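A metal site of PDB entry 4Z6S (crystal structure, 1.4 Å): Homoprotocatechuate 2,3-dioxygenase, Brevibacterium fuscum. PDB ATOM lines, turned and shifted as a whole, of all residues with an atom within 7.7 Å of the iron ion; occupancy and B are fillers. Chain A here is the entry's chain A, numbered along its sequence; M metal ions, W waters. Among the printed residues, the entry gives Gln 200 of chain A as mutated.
N of Glu 267 lies within hydrogen-bond range of O of Val 215 (2.9 Å). ND1 of His 155 sits at hydrogen-bond distance from OD2 of Asp 154, at 2.7 Å. N of Asn 157 lies within hydrogen-bond range of O of His 214 (2.9 Å). OH of Tyr 257 lies within hydrogen-bond range of OE2 of Glu 267, at 3.2 Å. The side-chain carboxylate (OE2) of Glu 267 lies within hydrogen-bond range of a ring nitrogen (NE2) of His 248 (2.8 Å). The backbone NH (N) of Ala 216 sits at hydrogen-bond distance from the backbone carbonyl oxygen (O) of His 155 (2.8 Å). NE2 of His 155 sits close to NE2 of Gln 200. A ring nitrogen (ND1) of His 214 is in hydrogen-bond range of a ring nitrogen (ND1) of His 213, 2.8 Å away.
Of the 21 residues printed, 3 come within 4 Å of the iron ion. The nearest printed residue that does not touch the iron ion is Gln 200 (4.01 Å).
The iron ion is bound by the side-chain carboxylate (OE1) of Glu 267 (2.1 Å), water W2 (2.1 Å), water W3 (2.2 Å), a ring nitrogen (NE2) of His 214 (2.2 Å), a ring nitrogen (NE2) of His 155 (2.2 Å) and water W1 (2.3 Å).
Water W2 lies within hydrogen-bond range of OE1 of Gln 200 and OE2 of Glu 267.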
ATOM      1  N   ASP A 154       3.677 -28.127 -34.874  1.00  0.00           N
ATOM      2  CA  ASP A 154       4.833 -28.941 -34.442  1.00  0.00           C
ATOM      3  C   ASP A 154       4.663 -29.759 -33.172  1.00  0.00           C
ATOM      4  O   ASP A 154       5.025 -30.942 -33.154  1.00  0.00           O
ATOM      5  CB  ASP A 154       6.117 -28.124 -34.280  1.00  0.00           C
ATOM      6  CG  ASP A 154       7.338 -29.033 -34.130  1.00  0.00           C
ATOM      7  OD1 ASP A 154       7.745 -29.689 -35.129  1.00  0.00           O
ATOM      8  OD2 ASP A 154       7.807 -29.190 -32.989  1.00  0.00           O
ATOM      9  N   HIS A 155       4.122 -29.143 -32.110  1.00  0.00           N
ATOM     10  CA  HIS A 155       4.021 -29.854 -30.843  1.00  0.00           C
ATOM     11  C   HIS A 155       3.123 -29.173 -29.852  1.00  0.00           C
ATOM     12  O   HIS A 155       2.728 -28.008 -30.005  1.00  0.00           O
ATOM     13  CB  HIS A 155       5.405 -30.068 -30.185  1.00  0.00           C
ATOM     14  CG  HIS A 155       6.114 -28.800 -29.782  1.00  0.00           C
ATOM     15  ND1 HIS A 155       7.018 -28.170 -30.598  1.00  0.00           N
ATOM     16  CD2 HIS A 155       6.123 -28.107 -28.613  1.00  0.00           C
ATOM     17  CE1 HIS A 155       7.523 -27.112 -29.965  1.00  0.00           C
ATOM     18  NE2 HIS A 155       7.021 -27.088 -28.749  1.00  0.00           N
ATOM     19  N   PHE A 156       2.838 -29.922 -28.790  1.00  0.00           N
ATOM     20  CA  PHE A 156       2.212 -29.423 -27.578  1.00  0.00           C
ATOM     21  C   PHE A 156       3.256 -29.438 -26.441  1.00  0.00           C
ATOM     22  O   PHE A 156       4.234 -30.188 -26.505  1.00  0.00           O
ATOM     23  CB  PHE A 156       1.049 -30.333 -27.151  1.00  0.00           C
ATOM     24  CG  PHE A 156       0.056 -30.641 -28.247  1.00  0.00           C
ATOM     25  CD1 PHE A 156      -0.602 -29.642 -28.952  1.00  0.00           C
ATOM     26  CD2 PHE A 156      -0.254 -31.963 -28.550  1.00  0.00           C
ATOM     27  CE1 PHE A 156      -1.530 -29.962 -29.930  1.00  0.00           C
ATOM     28  CE2 PHE A 156      -1.183 -32.293 -29.530  1.00  0.00           C
ATOM     29  CZ  PHE A 156      -1.791 -31.287 -30.235  1.00  0.00           C
ATOM     30  N   ASN A 157       3.000 -28.648 -25.398  1.00  0.00           N
ATOM     31  CA  ASN A 157       3.758 -28.750 -24.149  1.00  0.00           C
ATOM     32  C   ASN A 157       2.823 -28.673 -22.947  1.00  0.00           C
ATOM     33  O   ASN A 157       2.029 -27.730 -22.836  1.00  0.00           O
ATOM     34  CB  ASN A 157       4.824 -27.627 -24.110  1.00  0.00           C
ATOM     35  CG  ASN A 157       5.796 -27.761 -22.949  1.00  0.00           C
ATOM     36  OD1 ASN A 157       5.403 -27.767 -21.794  1.00  0.00           O
ATOM     37  ND2 ASN A 157       7.106 -27.860 -23.270  1.00  0.00           N
ATOM     38  N   TRP A 192      11.195 -33.994 -23.219  1.00  0.00           N
ATOM     39  CA  TRP A 192      10.659 -33.855 -24.554  1.00  0.00           C
ATOM     40  C   TRP A 192      10.549 -35.204 -25.196  1.00  0.00           C
ATOM     41  O   TRP A 192      11.443 -36.019 -25.044  1.00  0.00           O
ATOM     42  CB  TRP A 192      11.607 -32.995 -25.379  1.00  0.00           C
ATOM     43  CG  TRP A 192      11.590 -31.547 -25.011  1.00  0.00           C
ATOM     44  CD1 TRP A 192      10.983 -30.568 -25.743  1.00  0.00           C
ATOM     45  CD2 TRP A 192      12.183 -30.883 -23.866  1.00  0.00           C
ATOM     46  NE1 TRP A 192      11.145 -29.350 -25.138  1.00  0.00           N
ATOM     47  CE2 TRP A 192      11.889 -29.507 -23.990  1.00  0.00           C
ATOM     48  CE3 TRP A 192      12.950 -31.309 -22.764  1.00  0.00           C
ATOM     49  CZ2 TRP A 192      12.299 -28.549 -23.042  1.00  0.00           C
ATOM     50  CZ3 TRP A 192      13.365 -30.359 -21.826  1.00  0.00           C
ATOM     51  CH2 TRP A 192      13.045 -28.999 -21.969  1.00  0.00           C
ATOM     52  N   GLN A 200      10.026 -33.313 -30.776  1.00  0.00           N
ATOM     53  CA  GLN A 200       8.894 -33.456 -29.914  1.00  0.00           C
ATOM     54  C   GLN A 200       7.564 -33.472 -30.691  1.00  0.00           C
ATOM     55  O   GLN A 200       7.415 -32.799 -31.708  1.00  0.00           O
ATOM     56  CB  GLN A 200       8.915 -32.328 -28.891  1.00  0.00           C
ATOM     57  CG  GLN A 200       9.022 -30.933 -29.564  1.00  0.00           C
ATOM     58  CD  GLN A 200       9.254 -29.790 -28.613  1.00  0.00           C
ATOM     59  OE1 GLN A 200      10.111 -28.894 -28.863  1.00  0.00           O
ATOM     60  NE2 GLN A 200       8.530 -29.802 -27.530  1.00  0.00           N
ATOM     61  N   ALA A 203       5.555 -32.595 -24.789  1.00  0.00           N
ATOM     62  CA  ALA A 203       6.663 -32.339 -23.875  1.00  0.00           C
ATOM     63  C   ALA A 203       6.045 -32.084 -22.522  1.00  0.00           C
ATOM     64  O   ALA A 203       4.898 -31.638 -22.446  1.00  0.00           O
ATOM     65  CB  ALA A 203       7.476 -31.145 -24.347  1.00  0.00           C
ATOM     66  N   THR A 205       6.627 -30.161 -18.851  1.00  0.00           N
ATOM     67  CA  THR A 205       7.255 -29.124 -18.062  1.00  0.00           C
ATOM     68  C   THR A 205       6.780 -29.308 -16.614  1.00  0.00           C
ATOM     69  O   THR A 205       5.580 -29.339 -16.363  1.00  0.00           O
ATOM     70  CB  THR A 205       6.827 -27.726 -18.557  1.00  0.00           C
ATOM     71  OG1 THR A 205       7.293 -27.546 -19.902  1.00  0.00           O
ATOM     72  CG2 THR A 205       7.383 -26.642 -17.704  1.00  0.00           C
ATOM     73  N   HIS A 213       0.906 -25.766 -21.355  1.00  0.00           N
ATOM     74  CA  HIS A 213       1.914 -24.699 -21.460  1.00  0.00           C
ATOM     75  C   HIS A 213       1.838 -23.930 -22.759  1.00  0.00           C
ATOM     76  O   HIS A 213       1.737 -22.720 -22.740  1.00  0.00           O
ATOM     77  CB  HIS A 213       3.344 -25.233 -21.202  1.00  0.00           C
ATOM     78  CG  HIS A 213       4.297 -24.143 -20.879  1.00  0.00           C
ATOM     79  ND1 HIS A 213       4.845 -23.317 -21.824  1.00  0.00           N
ATOM     80  CD2 HIS A 213       4.759 -23.699 -19.686  1.00  0.00           C
ATOM     81  CE1 HIS A 213       5.599 -22.410 -21.253  1.00  0.00           C
ATOM     82  NE2 HIS A 213       5.565 -22.626 -19.943  1.00  0.00           N
ATOM     83  N   HIS A 214       1.872 -24.651 -23.889  1.00  0.00           N
ATOM     84  CA  HIS A 214       1.794 -24.022 -25.202  1.00  0.00           C
ATOM     85  C   HIS A 214       1.448 -24.994 -26.301  1.00  0.00           C
ATOM     86  O   HIS A 214       1.555 -26.221 -26.135  1.00  0.00           O
ATOM     87  CB  HIS A 214       3.054 -23.222 -25.547  1.00  0.00           C
ATOM     88  CG  HIS A 214       4.319 -24.025 -25.599  1.00  0.00           C
ATOM     89  ND1 HIS A 214       5.169 -24.119 -24.519  1.00  0.00           N
ATOM     90  CD2 HIS A 214       4.927 -24.683 -26.607  1.00  0.00           C
ATOM     91  CE1 HIS A 214       6.241 -24.826 -24.855  1.00  0.00           C
ATOM     92  NE2 HIS A 214       6.115 -25.204 -26.113  1.00  0.00           N
ATOM     93  N   VAL A 215       1.036 -24.397 -27.434  1.00  0.00           N
ATOM     94  CA  VAL A 215       0.966 -25.070 -28.705  1.00  0.00           C
ATOM     95  C   VAL A 215       1.999 -24.419 -29.600  1.00  0.00           C
ATOM     96  O   VAL A 215       2.092 -23.181 -29.590  1.00  0.00           O
ATOM     97  CB  VAL A 215      -0.454 -24.891 -29.319  1.00  0.00           C
ATOM     98  CG1 VAL A 215      -0.525 -25.520 -30.685  1.00  0.00           C
ATOM     99  CG2 VAL A 215      -1.486 -25.528 -28.386  1.00  0.00           C
ATOM    100  N   ALA A 216       2.770 -25.216 -30.361  1.00  0.00           N
ATOM    101  CA  ALA A 216       3.807 -24.661 -31.213  1.00  0.00           C
ATOM    102  C   ALA A 216       3.548 -24.899 -32.672  1.00  0.00           C
ATOM    103  O   ALA A 216       3.232 -26.033 -33.083  1.00  0.00           O
ATOM    104  CB  ALA A 216       5.173 -25.261 -30.822  1.00  0.00           C
ATOM    105  N   HIS A 248      16.940 -22.097 -28.824  1.00  0.00           N
ATOM    106  CA  HIS A 248      16.838 -23.030 -27.701  1.00  0.00           C
ATOM    107  C   HIS A 248      18.123 -23.828 -27.581  1.00  0.00           C
ATOM    108  O   HIS A 248      18.748 -24.125 -28.579  1.00  0.00           O
ATOM    109  CB  HIS A 248      15.729 -24.044 -27.918  1.00  0.00           C
ATOM    110  CG  HIS A 248      14.351 -23.536 -27.666  1.00  0.00           C
ATOM    111  ND1 HIS A 248      13.977 -22.898 -26.487  1.00  0.00           N
ATOM    112  CD2 HIS A 248      13.232 -23.673 -28.406  1.00  0.00           C
ATOM    113  CE1 HIS A 248      12.673 -22.644 -26.550  1.00  0.00           C
ATOM    114  NE2 HIS A 248      12.198 -23.136 -27.682  1.00  0.00           N
ATOM    115  N   SER A 251      16.546 -28.924 -28.054  1.00  0.00           N
ATOM    116  CA  SER A 251      15.924 -28.890 -29.396  1.00  0.00           C
ATOM    117  C   SER A 251      16.688 -28.141 -30.481  1.00  0.00           C
ATOM    118  O   SER A 251      16.512 -28.474 -31.672  1.00  0.00           O
ATOM    119  CB  SER A 251      14.467 -28.398 -29.409  1.00  0.00           C
ATOM    120  OG  SER A 251      14.413 -26.969 -29.532  1.00  0.00           O
ATOM    121  N   TYR A 255      13.116 -19.819 -31.848  1.00  0.00           N
ATOM    122  CA  TYR A 255      11.830 -19.807 -31.152  1.00  0.00           C
ATOM    123  C   TYR A 255      11.353 -18.410 -30.766  1.00  0.00           C
ATOM    124  O   TYR A 255      12.110 -17.437 -30.723  1.00  0.00           O
ATOM    125  CB  TYR A 255      11.902 -20.662 -29.888  1.00  0.00           C
ATOM    126  CG  TYR A 255      12.646 -19.997 -28.749  1.00  0.00           C
ATOM    127  CD1 TYR A 255      11.998 -19.133 -27.884  1.00  0.00           C
ATOM    128  CD2 TYR A 255      14.003 -20.238 -28.526  1.00  0.00           C
ATOM    129  CE1 TYR A 255      12.671 -18.499 -26.846  1.00  0.00           C
ATOM    130  CE2 TYR A 255      14.682 -19.625 -27.486  1.00  0.00           C
ATOM    131  CZ  TYR A 255      14.037 -18.736 -26.654  1.00  0.00           C
ATOM    132  OH  TYR A 255      14.723 -18.135 -25.609  1.00  0.00           O
ATOM    133  N   TYR A 257       7.790 -16.989 -28.087  1.00  0.00           N
ATOM    134  CA  TYR A 257       6.530 -17.254 -27.374  1.00  0.00           C
ATOM    135  C   TYR A 257       5.700 -15.969 -27.304  1.00  0.00           C
ATOM    136  O   TYR A 257       6.186 -14.940 -26.883  1.00  0.00           O
ATOM    137  CB  TYR A 257       6.796 -17.732 -25.941  1.00  0.00           C
ATOM    138  CG  TYR A 257       7.575 -19.024 -25.864  1.00  0.00           C
ATOM    139  CD1 TYR A 257       6.927 -20.252 -25.952  1.00  0.00           C
ATOM    140  CD2 TYR A 257       8.966 -18.994 -25.714  1.00  0.00           C
ATOM    141  CE1 TYR A 257       7.651 -21.448 -25.879  1.00  0.00           C
ATOM    142  CE2 TYR A 257       9.677 -20.180 -25.637  1.00  0.00           C
ATOM    143  CZ  TYR A 257       9.026 -21.388 -25.714  1.00  0.00           C
ATOM    144  OH  TYR A 257       9.782 -22.563 -25.666  1.00  0.00           O
ATOM    145  N   GLU A 267       3.910 -20.947 -29.268  1.00  0.00           N
ATOM    146  CA  GLU A 267       5.312 -20.894 -29.633  1.00  0.00           C
ATOM    147  C   GLU A 267       5.412 -20.938 -31.142  1.00  0.00           C
ATOM    148  O   GLU A 267       4.653 -21.667 -31.823  1.00  0.00           O
ATOM    149  CB  GLU A 267       6.085 -22.066 -29.049  1.00  0.00           C
ATOM    150  CG  GLU A 267       7.572 -22.029 -29.345  1.00  0.00           C
ATOM    151  CD  GLU A 267       8.330 -23.205 -28.795  1.00  0.00           C
ATOM    152  OE1 GLU A 267       7.693 -24.149 -28.324  1.00  0.00           O
ATOM    153  OE2 GLU A 267       9.583 -23.183 -28.803  1.00  0.00           O
ATOM    154  N   ILE A 268       6.341 -20.159 -31.671  1.00  0.00           N
ATOM    155  CA  ILE A 268       6.730 -20.268 -33.083  1.00  0.00           C
ATOM    156  C   ILE A 268       8.147 -20.826 -33.080  1.00  0.00           C
ATOM    157  O   ILE A 268       8.977 -20.416 -32.259  1.00  0.00           O
ATOM    158  CB  ILE A 268       6.715 -18.905 -33.820  1.00  0.00           C
ATOM    159  CG1 ILE A 268       5.512 -18.015 -33.423  1.00  0.00           C
ATOM    160  CG2 ILE A 268       6.729 -19.137 -35.320  1.00  0.00           C
ATOM    161  CD1 ILE A 268       4.156 -18.601 -33.674  1.00  0.00           C
ATOM    162  N   TYR A 269       8.423 -21.780 -33.979  1.00  0.00           N
ATOM    163  CA  TYR A 269       9.539 -22.705 -33.804  1.00  0.00           C
ATOM    164  C   TYR A 269      10.104 -23.075 -35.181  1.00  0.00           C
ATOM    165  O   TYR A 269       9.347 -23.228 -36.135  1.00  0.00           O
ATOM    166  CB  TYR A 269       8.947 -23.927 -33.109  1.00  0.00           C
ATOM    167  CG  TYR A 269       9.804 -25.107 -32.723  1.00  0.00           C
ATOM    168  CD1 TYR A 269      10.344 -25.228 -31.445  1.00  0.00           C
ATOM    169  CD2 TYR A 269       9.916 -26.177 -33.588  1.00  0.00           C
ATOM    170  CE1 TYR A 269      11.008 -26.385 -31.057  1.00  0.00           C
ATOM    171  CE2 TYR A 269      10.603 -27.320 -33.231  1.00  0.00           C
ATOM    172  CZ  TYR A 269      11.157 -27.410 -31.964  1.00  0.00           C
ATOM    173  OH  TYR A 269      11.779 -28.565 -31.568  1.00  0.00           O
ATOM    174  N   ARG A 293      17.957 -23.349 -22.086  1.00  0.00           N
ATOM    175  CA  ARG A 293      16.620 -22.938 -22.584  1.00  0.00           C
ATOM    176  C   ARG A 293      16.750 -21.871 -23.663  1.00  0.00           C
ATOM    177  O   ARG A 293      16.108 -21.938 -24.712  1.00  0.00           O
ATOM    178  CB  ARG A 293      15.735 -22.473 -21.433  1.00  0.00           C
ATOM    179  CG  ARG A 293      15.213 -23.637 -20.610  1.00  0.00           C
ATOM    180  CD  ARG A 293      13.965 -23.326 -19.824  1.00  0.00           C
ATOM    181  NE  ARG A 293      13.414 -24.467 -19.079  1.00  0.00           N
ATOM    182  CZ  ARG A 293      12.563 -25.360 -19.558  1.00  0.00           C
ATOM    183  NH1 ARG A 293      12.164 -25.321 -20.832  1.00  0.00           N
ATOM    184  NH2 ARG A 293      12.086 -26.298 -18.781  1.00  0.00           N
ATOM    185  N   TRP A 304       6.963 -17.456 -17.854  1.00  0.00           N
ATOM    186  CA  TRP A 304       7.121 -18.683 -18.628  1.00  0.00           C
ATOM    187  C   TRP A 304       7.048 -19.903 -17.708  1.00  0.00           C
ATOM    188  O   TRP A 304       6.562 -20.969 -18.084  1.00  0.00           O
ATOM    189  CB  TRP A 304       8.450 -18.655 -19.413  1.00  0.00           C
ATOM    190  CG  TRP A 304       8.440 -19.571 -20.580  1.00  0.00           C
ATOM    191  CD1 TRP A 304       8.023 -19.287 -21.856  1.00  0.00           C
ATOM    192  CD2 TRP A 304       8.838 -20.945 -20.592  1.00  0.00           C
ATOM    193  NE1 TRP A 304       8.125 -20.406 -22.646  1.00  0.00           N
ATOM    194  CE2 TRP A 304       8.632 -21.431 -21.903  1.00  0.00           C
ATOM    195  CE3 TRP A 304       9.329 -21.817 -19.625  1.00  0.00           C
ATOM    196  CZ2 TRP A 304       8.903 -22.747 -22.253  1.00  0.00           C
ATOM    197  CZ3 TRP A 304       9.593 -23.112 -19.978  1.00  0.00           C
ATOM    198  CH2 TRP A 304       9.370 -23.569 -21.274  1.00  0.00           C
HETATM  199 FE    FE M   1       7.939 -25.852 -27.167  1.00  0.00          FE
HETATM  200  O   HOH W   1       8.211 -27.749 -25.935  1.00  0.00           O
HETATM  201  O   HOH W   2       9.905 -26.147 -27.857  1.00  0.00           O
HETATM  202  O   HOH W   3       9.100 -24.894 -25.600  1.00  0.00           O
